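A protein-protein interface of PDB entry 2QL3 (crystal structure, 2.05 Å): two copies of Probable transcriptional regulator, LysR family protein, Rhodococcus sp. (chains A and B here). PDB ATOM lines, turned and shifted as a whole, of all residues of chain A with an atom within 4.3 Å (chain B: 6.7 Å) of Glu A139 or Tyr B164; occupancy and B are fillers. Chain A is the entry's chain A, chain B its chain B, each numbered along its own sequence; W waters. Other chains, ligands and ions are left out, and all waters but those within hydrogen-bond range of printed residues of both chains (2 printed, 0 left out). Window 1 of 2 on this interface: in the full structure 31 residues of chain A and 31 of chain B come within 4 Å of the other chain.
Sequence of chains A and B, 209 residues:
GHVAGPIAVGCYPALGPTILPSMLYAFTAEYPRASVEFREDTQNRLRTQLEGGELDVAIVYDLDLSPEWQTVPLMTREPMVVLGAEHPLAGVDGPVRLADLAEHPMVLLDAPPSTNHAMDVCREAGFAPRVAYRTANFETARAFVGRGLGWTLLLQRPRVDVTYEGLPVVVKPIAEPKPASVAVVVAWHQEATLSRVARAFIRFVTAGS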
ATOM      1  N   PRO A  17      16.507   5.964 -10.346  1.00  0.00           N
ATOM      2  CA  PRO A  17      17.404   4.870  -9.804  1.00  0.00           C
ATOM      3  C   PRO A  17      17.872   3.789 -10.793  1.00  0.00           C
ATOM      4  O   PRO A  17      18.735   2.995 -10.481  1.00  0.00           O
ATOM      5  CB  PRO A  17      16.551   4.207  -8.725  1.00  0.00           C
ATOM      6  CG  PRO A  17      15.126   4.638  -8.993  1.00  0.00           C
ATOM      7  CD  PRO A  17      15.078   5.688 -10.078  1.00  0.00           C
ATOM      8  N   THR A  18      17.316   3.786 -12.001  1.00  0.00           N
ATOM      9  CA  THR A  18      17.542   2.672 -12.910  1.00  0.00           C
ATOM     10  C   THR A  18      18.541   3.075 -13.984  1.00  0.00           C
ATOM     11  O   THR A  18      19.505   2.331 -14.247  1.00  0.00           O
ATOM     12  CB  THR A  18      16.240   2.191 -13.558  1.00  0.00           C
ATOM     13  OG1 THR A  18      15.579   3.313 -14.133  1.00  0.00           O
ATOM     14  CG2 THR A  18      15.298   1.658 -12.509  1.00  0.00           C
ATOM     15  N   ASN A 137       4.677   5.609  -6.704  1.00  0.00           N
ATOM     16  CA  ASN A 137       5.987   5.147  -6.258  1.00  0.00           C
ATOM     17  C   ASN A 137       6.325   3.762  -6.820  1.00  0.00           C
ATOM     18  O   ASN A 137       5.628   2.829  -6.573  1.00  0.00           O
ATOM     19  CB  ASN A 137       6.040   5.107  -4.751  1.00  0.00           C
ATOM     20  CG  ASN A 137       7.473   4.908  -4.225  1.00  0.00           C
ATOM     21  OD1 ASN A 137       8.454   5.168  -4.939  1.00  0.00           O
ATOM     22  ND2 ASN A 137       7.593   4.460  -2.992  1.00  0.00           N
ATOM     23  N   PHE A 138       7.386   3.651  -7.595  1.00  0.00           N
ATOM     24  CA  PHE A 138       7.720   2.397  -8.284  1.00  0.00           C
ATOM     25  C   PHE A 138       7.906   1.260  -7.313  1.00  0.00           C
ATOM     26  O   PHE A 138       7.417   0.165  -7.545  1.00  0.00           O
ATOM     27  CB  PHE A 138       8.980   2.614  -9.122  1.00  0.00           C
ATOM     28  CG  PHE A 138       9.265   1.590 -10.142  1.00  0.00           C
ATOM     29  CD1 PHE A 138       8.886   1.792 -11.466  1.00  0.00           C
ATOM     30  CD2 PHE A 138      10.069   0.504  -9.846  1.00  0.00           C
ATOM     31  CE1 PHE A 138       9.219   0.852 -12.488  1.00  0.00           C
ATOM     32  CE2 PHE A 138      10.390  -0.422 -10.843  1.00  0.00           C
ATOM     33  CZ  PHE A 138       9.951  -0.261 -12.152  1.00  0.00           C
ATOM     34  N   GLU A 139       8.644   1.509  -6.246  1.00  0.00           N
ATOM     35  CA  GLU A 139       8.904   0.445  -5.274  1.00  0.00           C
ATOM     36  C   GLU A 139       7.665   0.087  -4.483  1.00  0.00           C
ATOM     37  O   GLU A 139       7.508  -1.063  -4.084  1.00  0.00           O
ATOM     38  CB  GLU A 139      10.007   0.815  -4.307  1.00  0.00           C
ATOM     39  CG  GLU A 139      10.415  -0.360  -3.382  1.00  0.00           C
ATOM     40  CD  GLU A 139      10.878  -1.628  -4.134  1.00  0.00           C
ATOM     41  OE1 GLU A 139      10.909  -2.711  -3.512  1.00  0.00           O
ATOM     42  OE2 GLU A 139      11.204  -1.566  -5.350  1.00  0.00           O
ATOM     43  N   THR A 140       6.779   1.053  -4.250  1.00  0.00           N
ATOM     44  CA  THR A 140       5.538   0.704  -3.617  1.00  0.00           C
ATOM     45  C   THR A 140       4.756  -0.304  -4.480  1.00  0.00           C
ATOM     46  O   THR A 140       4.174  -1.261  -3.951  1.00  0.00           O
ATOM     47  CB  THR A 140       4.698   1.940  -3.265  1.00  0.00           C
ATOM     48  OG1 THR A 140       5.449   2.774  -2.360  1.00  0.00           O
ATOM     49  CG2 THR A 140       3.350   1.514  -2.626  1.00  0.00           C
ATOM     50  N   ALA A 141       4.775  -0.122  -5.801  1.00  0.00           N
ATOM     51  CA  ALA A 141       4.078  -1.039  -6.681  1.00  0.00           C
ATOM     52  C   ALA A 141       4.703  -2.419  -6.561  1.00  0.00           C
ATOM     53  O   ALA A 141       3.995  -3.382  -6.420  1.00  0.00           O
ATOM     54  CB  ALA A 141       4.115  -0.568  -8.133  1.00  0.00           C
ATOM     55  N   ARG A 142       6.024  -2.512  -6.659  1.00  0.00           N
ATOM     56  CA  ARG A 142       6.743  -3.820  -6.557  1.00  0.00           C
ATOM     57  C   ARG A 142       6.545  -4.434  -5.208  1.00  0.00           C
ATOM     58  O   ARG A 142       6.259  -5.650  -5.128  1.00  0.00           O
ATOM     59  CB  ARG A 142       8.262  -3.656  -6.776  1.00  0.00           C
ATOM     60  CG  ARG A 142       8.649  -3.230  -8.149  1.00  0.00           C
ATOM     61  CD  ARG A 142      10.186  -3.042  -8.260  1.00  0.00           C
ATOM     62  NE  ARG A 142      10.870  -4.338  -8.341  1.00  0.00           N
ATOM     63  CZ  ARG A 142      11.722  -4.821  -7.451  1.00  0.00           C
ATOM     64  NH1 ARG A 142      12.305  -5.998  -7.671  1.00  0.00           N
ATOM     65  NH2 ARG A 142      12.007  -4.150  -6.355  1.00  0.00           N
ATOM     66  N   ALA A 143       6.629  -3.622  -4.148  1.00  0.00           N
ATOM     67  CA  ALA A 143       6.467  -4.159  -2.781  1.00  0.00           C
ATOM     68  C   ALA A 143       5.049  -4.689  -2.518  1.00  0.00           C
ATOM     69  O   ALA A 143       4.892  -5.742  -1.889  1.00  0.00           O
ATOM     70  CB  ALA A 143       6.807  -3.124  -1.758  1.00  0.00           C
ATOM     71  N   PRO A 158      14.195  -3.698 -11.948  1.00  0.00           N
ATOM     72  CA  PRO A 158      15.359  -3.707 -11.043  1.00  0.00           C
ATOM     73  C   PRO A 158      16.176  -4.976 -11.189  1.00  0.00           C
ATOM     74  O   PRO A 158      15.619  -6.068 -11.374  1.00  0.00           O
ATOM     75  CB  PRO A 158      14.731  -3.613  -9.652  1.00  0.00           C
ATOM     76  CG  PRO A 158      13.475  -2.804  -9.910  1.00  0.00           C
ATOM     77  CD  PRO A 158      12.950  -3.310 -11.249  1.00  0.00           C
ATOM     78  N   ARG A 159      17.486  -4.844 -11.057  1.00  0.00           N
ATOM     79  CA  ARG A 159      18.373  -5.988 -11.307  1.00  0.00           C
ATOM     80  C   ARG A 159      18.179  -7.216 -10.431  1.00  0.00           C
ATOM     81  O   ARG A 159      18.439  -8.346 -10.893  1.00  0.00           O
ATOM     82  CB  ARG A 159      19.853  -5.557 -11.326  1.00  0.00           C
ATOM     83  CG  ARG A 159      20.543  -6.056 -12.635  1.00  0.00           C
ATOM     84  CD  ARG A 159      21.731  -5.226 -13.126  1.00  0.00           C
ATOM     85  NE  ARG A 159      21.515  -4.557 -14.411  1.00  0.00           N
ATOM     86  CZ  ARG A 159      21.927  -3.313 -14.684  1.00  0.00           C
ATOM     87  NH1 ARG A 159      22.549  -2.590 -13.759  1.00  0.00           N
ATOM     88  NH2 ARG A 159      21.708  -2.768 -15.882  1.00  0.00           N
ATOM     89  N   THR A 163      11.987  -7.036  -3.147  1.00  0.00           N
ATOM     90  CA  THR A 163      11.379  -5.800  -2.777  1.00  0.00           C
ATOM     91  C   THR A 163      12.038  -5.331  -1.500  1.00  0.00           C
ATOM     92  O   THR A 163      12.886  -6.057  -0.925  1.00  0.00           O
ATOM     93  CB  THR A 163       9.854  -5.942  -2.548  1.00  0.00           C
ATOM     94  OG1 THR A 163       9.631  -6.621  -1.304  1.00  0.00           O
ATOM     95  CG2 THR A 163       9.112  -6.700  -3.715  1.00  0.00           C
ATOM     96  N   TYR A 164      11.642  -4.151  -1.012  1.00  0.00           N
ATOM     97  CA  TYR A 164      12.195  -3.640   0.258  1.00  0.00           C
ATOM     98  C   TYR A 164      11.884  -4.504   1.485  1.00  0.00           C
ATOM     99  O   TYR A 164      12.611  -4.453   2.460  1.00  0.00           O
ATOM    100  CB  TYR A 164      11.701  -2.208   0.554  1.00  0.00           C
ATOM    101  CG  TYR A 164      12.353  -1.048  -0.228  1.00  0.00           C
ATOM    102  CD1 TYR A 164      11.932   0.273  -0.007  1.00  0.00           C
ATOM    103  CD2 TYR A 164      13.369  -1.271  -1.174  1.00  0.00           C
ATOM    104  CE1 TYR A 164      12.540   1.348  -0.661  1.00  0.00           C
ATOM    105  CE2 TYR A 164      13.977  -0.208  -1.852  1.00  0.00           C
ATOM    106  CZ  TYR A 164      13.558   1.096  -1.584  1.00  0.00           C
ATOM    107  OH  TYR A 164      14.157   2.137  -2.232  1.00  0.00           O
ATOM    108  N   GLY B  16       5.391   3.589   2.166  1.00  0.00           N
ATOM    109  CA  GLY B  16       4.635   2.709   1.273  1.00  0.00           C
ATOM    110  C   GLY B  16       5.219   1.329   0.990  1.00  0.00           C
ATOM    111  O   GLY B  16       4.518   0.337   1.111  1.00  0.00           O
ATOM    112  N   PRO B  17       6.525   1.259   0.629  1.00  0.00           N
ATOM    113  CA  PRO B  17       7.088  -0.043   0.335  1.00  0.00           C
ATOM    114  C   PRO B  17       7.678  -0.771   1.539  1.00  0.00           C
ATOM    115  O   PRO B  17       7.929  -1.965   1.462  1.00  0.00           O
ATOM    116  CB  PRO B  17       8.159   0.259  -0.745  1.00  0.00           C
ATOM    117  CG  PRO B  17       8.520   1.705  -0.567  1.00  0.00           C
ATOM    118  CD  PRO B  17       7.519   2.339   0.421  1.00  0.00           C
ATOM    119  N   THR B  18       7.833  -0.069   2.664  1.00  0.00           N
ATOM    120  CA  THR B  18       8.510  -0.617   3.853  1.00  0.00           C
ATOM    121  C   THR B  18       7.524  -1.116   4.909  1.00  0.00           C
ATOM    122  O   THR B  18       7.686  -2.180   5.405  1.00  0.00           O
ATOM    123  CB  THR B  18       9.483   0.408   4.517  1.00  0.00           C
ATOM    124  OG1 THR B  18       8.765   1.588   4.882  1.00  0.00           O
ATOM    125  CG2 THR B  18      10.613   0.845   3.586  1.00  0.00           C
ATOM    126  N   PRO B  21       2.975  -2.678   2.993  1.00  0.00           N
ATOM    127  CA  PRO B  21       2.495  -3.867   2.277  1.00  0.00           C
ATOM    128  C   PRO B  21       2.029  -4.968   3.246  1.00  0.00           C
ATOM    129  O   PRO B  21       0.943  -5.503   3.035  1.00  0.00           O
ATOM    130  CB  PRO B  21       3.743  -4.336   1.465  1.00  0.00           C
ATOM    131  CG  PRO B  21       4.567  -3.039   1.310  1.00  0.00           C
ATOM    132  CD  PRO B  21       4.392  -2.387   2.656  1.00  0.00           C
ATOM    133  N   ASN B 137      13.006  10.725  -4.036  1.00  0.00           N
ATOM    134  CA  ASN B 137      12.831   9.295  -4.305  1.00  0.00           C
ATOM    135  C   ASN B 137      13.832   8.455  -3.492  1.00  0.00           C
ATOM    136  O   ASN B 137      15.035   8.508  -3.734  1.00  0.00           O
ATOM    137  CB  ASN B 137      13.002   9.061  -5.836  1.00  0.00           C
ATOM    138  CG  ASN B 137      12.469   7.717  -6.316  1.00  0.00           C
ATOM    139  OD1 ASN B 137      11.526   7.178  -5.738  1.00  0.00           O
ATOM    140  ND2 ASN B 137      12.979   7.235  -7.451  1.00  0.00           N
ATOM    141  N   GLU B 139      14.658   5.294  -3.503  1.00  0.00           N
ATOM    142  CA  GLU B 139      15.528   4.433  -4.270  1.00  0.00           C
ATOM    143  C   GLU B 139      16.542   5.243  -5.064  1.00  0.00           C
ATOM    144  O   GLU B 139      17.640   4.773  -5.336  1.00  0.00           O
ATOM    145  CB  GLU B 139      14.781   3.461  -5.208  1.00  0.00           C
ATOM    146  CG  GLU B 139      15.765   2.405  -5.853  1.00  0.00           C
ATOM    147  CD  GLU B 139      16.581   1.491  -4.821  1.00  0.00           C
ATOM    148  OE1 GLU B 139      17.548   0.857  -5.270  1.00  0.00           O
ATOM    149  OE2 GLU B 139      16.297   1.458  -3.584  1.00  0.00           O
ATOM    150  N   ARG B 142      19.337   5.750  -2.696  1.00  0.00           N
ATOM    151  CA  ARG B 142      20.108   4.504  -2.544  1.00  0.00           C
ATOM    152  C   ARG B 142      20.985   4.172  -3.770  1.00  0.00           C
ATOM    153  O   ARG B 142      22.131   3.789  -3.607  1.00  0.00           O
ATOM    154  CB  ARG B 142      19.172   3.348  -2.246  1.00  0.00           C
ATOM    155  CG  ARG B 142      18.647   3.493  -0.823  1.00  0.00           C
ATOM    156  CD  ARG B 142      17.815   2.317  -0.431  1.00  0.00           C
ATOM    157  NE  ARG B 142      18.573   1.124   0.001  1.00  0.00           N
ATOM    158  CZ  ARG B 142      18.663   0.030  -0.732  1.00  0.00           C
ATOM    159  NH1 ARG B 142      19.343  -1.018  -0.256  1.00  0.00           N
ATOM    160  NH2 ARG B 142      18.065  -0.012  -1.955  1.00  0.00           N
ATOM    161  N   ALA B 143      20.405   4.278  -4.959  1.00  0.00           N
ATOM    162  CA  ALA B 143      21.103   3.957  -6.223  1.00  0.00           C
ATOM    163  C   ALA B 143      22.283   4.878  -6.457  1.00  0.00           C
ATOM    164  O   ALA B 143      23.349   4.440  -6.868  1.00  0.00           O
ATOM    165  CB  ALA B 143      20.136   4.043  -7.413  1.00  0.00           C
ATOM    166  N   VAL B 162      21.029  -3.708  -1.640  1.00  0.00           N
ATOM    167  CA  VAL B 162      21.349  -3.651  -3.055  1.00  0.00           C
ATOM    168  C   VAL B 162      20.393  -2.655  -3.643  1.00  0.00           C
ATOM    169  O   VAL B 162      19.323  -2.467  -3.128  1.00  0.00           O
ATOM    170  CB  VAL B 162      21.178  -5.069  -3.740  1.00  0.00           C
ATOM    171  CG1 VAL B 162      19.723  -5.476  -3.964  1.00  0.00           C
ATOM    172  CG2 VAL B 162      21.997  -5.191  -5.025  1.00  0.00           C
ATOM    173  N   THR B 163      20.794  -2.035  -4.740  1.00  0.00           N
ATOM    174  CA  THR B 163      19.998  -1.089  -5.507  1.00  0.00           C
ATOM    175  C   THR B 163      19.414  -1.705  -6.737  1.00  0.00           C
ATOM    176  O   THR B 163      19.755  -2.818  -7.141  1.00  0.00           O
ATOM    177  CB  THR B 163      20.863   0.100  -5.934  1.00  0.00           C
ATOM    178  OG1 THR B 163      21.772  -0.308  -6.982  1.00  0.00           O
ATOM    179  CG2 THR B 163      21.634   0.600  -4.689  1.00  0.00           C
ATOM    180  N   TYR B 164      18.488  -0.965  -7.313  1.00  0.00           N
ATOM    181  CA  TYR B 164      17.880  -1.292  -8.581  1.00  0.00           C
ATOM    182  C   TYR B 164      18.911  -1.614  -9.644  1.00  0.00           C
ATOM    183  O   TYR B 164      18.644  -2.404 -10.512  1.00  0.00           O
ATOM    184  CB  TYR B 164      17.035  -0.094  -9.019  1.00  0.00           C
ATOM    185  CG  TYR B 164      15.645  -0.025  -8.401  1.00  0.00           C
ATOM    186  CD1 TYR B 164      14.700   0.850  -8.946  1.00  0.00           C
ATOM    187  CD2 TYR B 164      15.278  -0.827  -7.307  1.00  0.00           C
ATOM    188  CE1 TYR B 164      13.444   0.957  -8.445  1.00  0.00           C
ATOM    189  CE2 TYR B 164      13.990  -0.701  -6.748  1.00  0.00           C
ATOM    190  CZ  TYR B 164      13.092   0.210  -7.365  1.00  0.00           C
ATOM    191  OH  TYR B 164      11.852   0.358  -6.891  1.00  0.00           O
ATOM    192  N   GLU B 165      20.104  -1.005  -9.548  1.00  0.00           N
ATOM    193  CA  GLU B 165      21.200  -1.236 -10.507  1.00  0.00           C
ATOM    194  C   GLU B 165      21.959  -2.525 -10.226  1.00  0.00           C
ATOM    195  O   GLU B 165      22.764  -2.949 -11.059  1.00  0.00           O
ATOM    196  CB  GLU B 165      22.209  -0.067 -10.475  1.00  0.00           C
ATOM    197  CG  GLU B 165      21.722   1.209 -11.084  1.00  0.00           C
ATOM    198  CD  GLU B 165      22.856   2.201 -11.314  1.00  0.00           C
ATOM    199  OE1 GLU B 165      23.621   2.461 -10.335  1.00  0.00           O
ATOM    200  OE2 GLU B 165      23.000   2.704 -12.458  1.00  0.00           O
ATOM    201  N   GLY B 166      21.706  -3.143  -9.066  1.00  0.00           N
ATOM    202  CA  GLY B 166      22.421  -4.370  -8.672  1.00  0.00           C
ATOM    203  C   GLY B 166      23.744  -4.087  -7.951  1.00  0.00           C
ATOM    204  O   GLY B 166      24.604  -4.960  -7.860  1.00  0.00           O
ATOM    205  N   LEU B 167      23.918  -2.870  -7.435  1.00  0.00           N
ATOM    206  CA  LEU B 167      25.130  -2.539  -6.680  1.00  0.00           C
ATOM    207  C   LEU B 167      24.851  -2.615  -5.167  1.00  0.00           C
ATOM    208  O   LEU B 167      23.730  -2.363  -4.719  1.00  0.00           O
ATOM    209  CB  LEU B 167      25.707  -1.164  -7.082  1.00  0.00           C
ATOM    210  CG  LEU B 167      26.208  -1.097  -8.550  1.00  0.00           C
ATOM    211  CD1 LEU B 167      26.733   0.332  -8.861  1.00  0.00           C
ATOM    212  CD2 LEU B 167      27.265  -2.126  -8.874  1.00  0.00           C
HETATM  213  O   HOH W   1      17.647  -4.506  -7.868  1.00  0.00           O
HETATM  214  O   HOH W   2      11.185   3.336  -6.314  1.00  0.00           O
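ND2 of Asn A137 sits at hydrogen-bond distance from OG1 of Thr A140, at 2.8 Å.
OE2 of Glu A139 is in salt-bridge range of NH2 of Arg A142, at 2.9 Å.
N of Tyr B164 lies within hydrogen-bond range of OE1 of Glu B139 (2.9 Å).
The side-chain carboxylate (OE1) of Glu A139 is in hydrogen-bond range of the backbone NH (N) of Tyr A164 (3.0 Å).
The side-chain carboxylate (OE2) of Glu B139 is in salt-bridge range of the guanidinium group (NH2) of Arg B142.
OG1 of Thr B163 sits close to N of Glu B165, 3.1 Å away.
NH1 of Arg A159 is in hydrogen-bond range of O of Glu B165 (2.7 Å).
OE2 of Glu A139 lies within hydrogen-bond range of OH of Tyr B164 (2.5 Å).
The backbone carbonyl oxygen (O) of Tyr B164 is in hydrogen-bond range of the backbone NH (N) of Arg A159 (2.8 Å).
OH of Tyr A164 is in hydrogen-bond range of OE2 of Glu B139 (2.6 Å).
Pro A17 touches Ala B143, and with the chains exchanged Ala A143 touches Pro B17.
Pro A17 touches Tyr B164, and with the chains exchanged Tyr A164 touches Pro B17.
Glu A139 touches Tyr B164, and with the chains exchanged Tyr A164 touches Glu B139.
Arg A142 touches Tyr B164, but with the chains exchanged Tyr A164 does not touch Arg B142 (4.1 Å).
Of the 24 pairs that touch across the chains among the printed residues, 13 have their exchanged pair printed and touching as well.
Water W1 lies within hydrogen-bond range of the backbone carbonyl oxygen (O) of Thr B163 (2.8 Å) and the backbone NH (N) of Arg A159 (3.2 Å).
Water W2 lies within hydrogen-bond range of the side-chain hydroxyl (OH) of Tyr B164 and the backbone NH (N) of Glu A139.
Among the printed residues, pairs that only touch across the chains: Phe A138 with Tyr B164 (3.5 Å), Pro A17 with Glu B139 (3.5 Å), Thr A140 with Pro B17 (3.5 Å), Glu A139 with Pro B17 (3.5 Å), Pro A17 with Ala B143 (3.5 Å), Pro A17 with Glu B165 (3.5 Å), Pro A158 with Tyr B164 (3.6 Å), Ala A143 with Pro B17 (3.6 Å), Thr A140 with Gly B16 (3.7 Å), Pro A17 with Asn B137 (3.7 Å), Thr A18 with Tyr B164 (3.7 Å), Tyr A164 with Pro B17 (3.7 Å), Asn A137 with Asn B137 (3.8 Å), Asn A137 with Pro B17 (3.8 Å), Arg A159 with Gly B166 (3.8 Å), Ala A143 with Pro B21 (3.8 Å), Pro A17 with Tyr B164 (3.8 Å), Tyr A164 with Thr B18 (3.9 Å), Thr A18 with Glu B165 (3.9 Å) and Arg A142 with Tyr B164 (3.998 Å).
Of the 14 printed residues of chain B, 10 touch a printed residue of chain A.
Of the 13 printed residues of chain A, 11 touch a printed residue of chain B.
Hydrophobic or aromatic side chains of chain A within 4 Å of the printed part of chain B: Pro A17, Phe A138, Ala A143, Pro A158 and Tyr A164.
Among the printed residues, no Asp or Glu carboxylate lies within 4 Å of a Lys or Arg side-chain nitrogen of the other chain.
Printed residues of chain B within 4 Å of Glu A139: Pro B17 and Tyr B164.
Ala A141 touches none of the printed residues of chain B.
Of the printed residues of chain B, Pro A158 touches Tyr B164 (3.6 Å).
Printed residues of chain B within 4 Å of Arg A159: Tyr B164, Glu B165 and Gly B166.
Thr A163 touches none of the printed residues of chain B.
Printed residues of chain A within 4 Å of Gly B16: Thr A140.
Of the printed residues of chain A, Tyr B164 touches Pro A17 (3.8 Å), Thr A18 (3.7 Å), Phe A138 (3.5 Å), Glu A139 (2.5 Å), Arg A142 (3.998 Å), Pro A158 (3.6 Å) and Arg A159 (2.8 Å).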
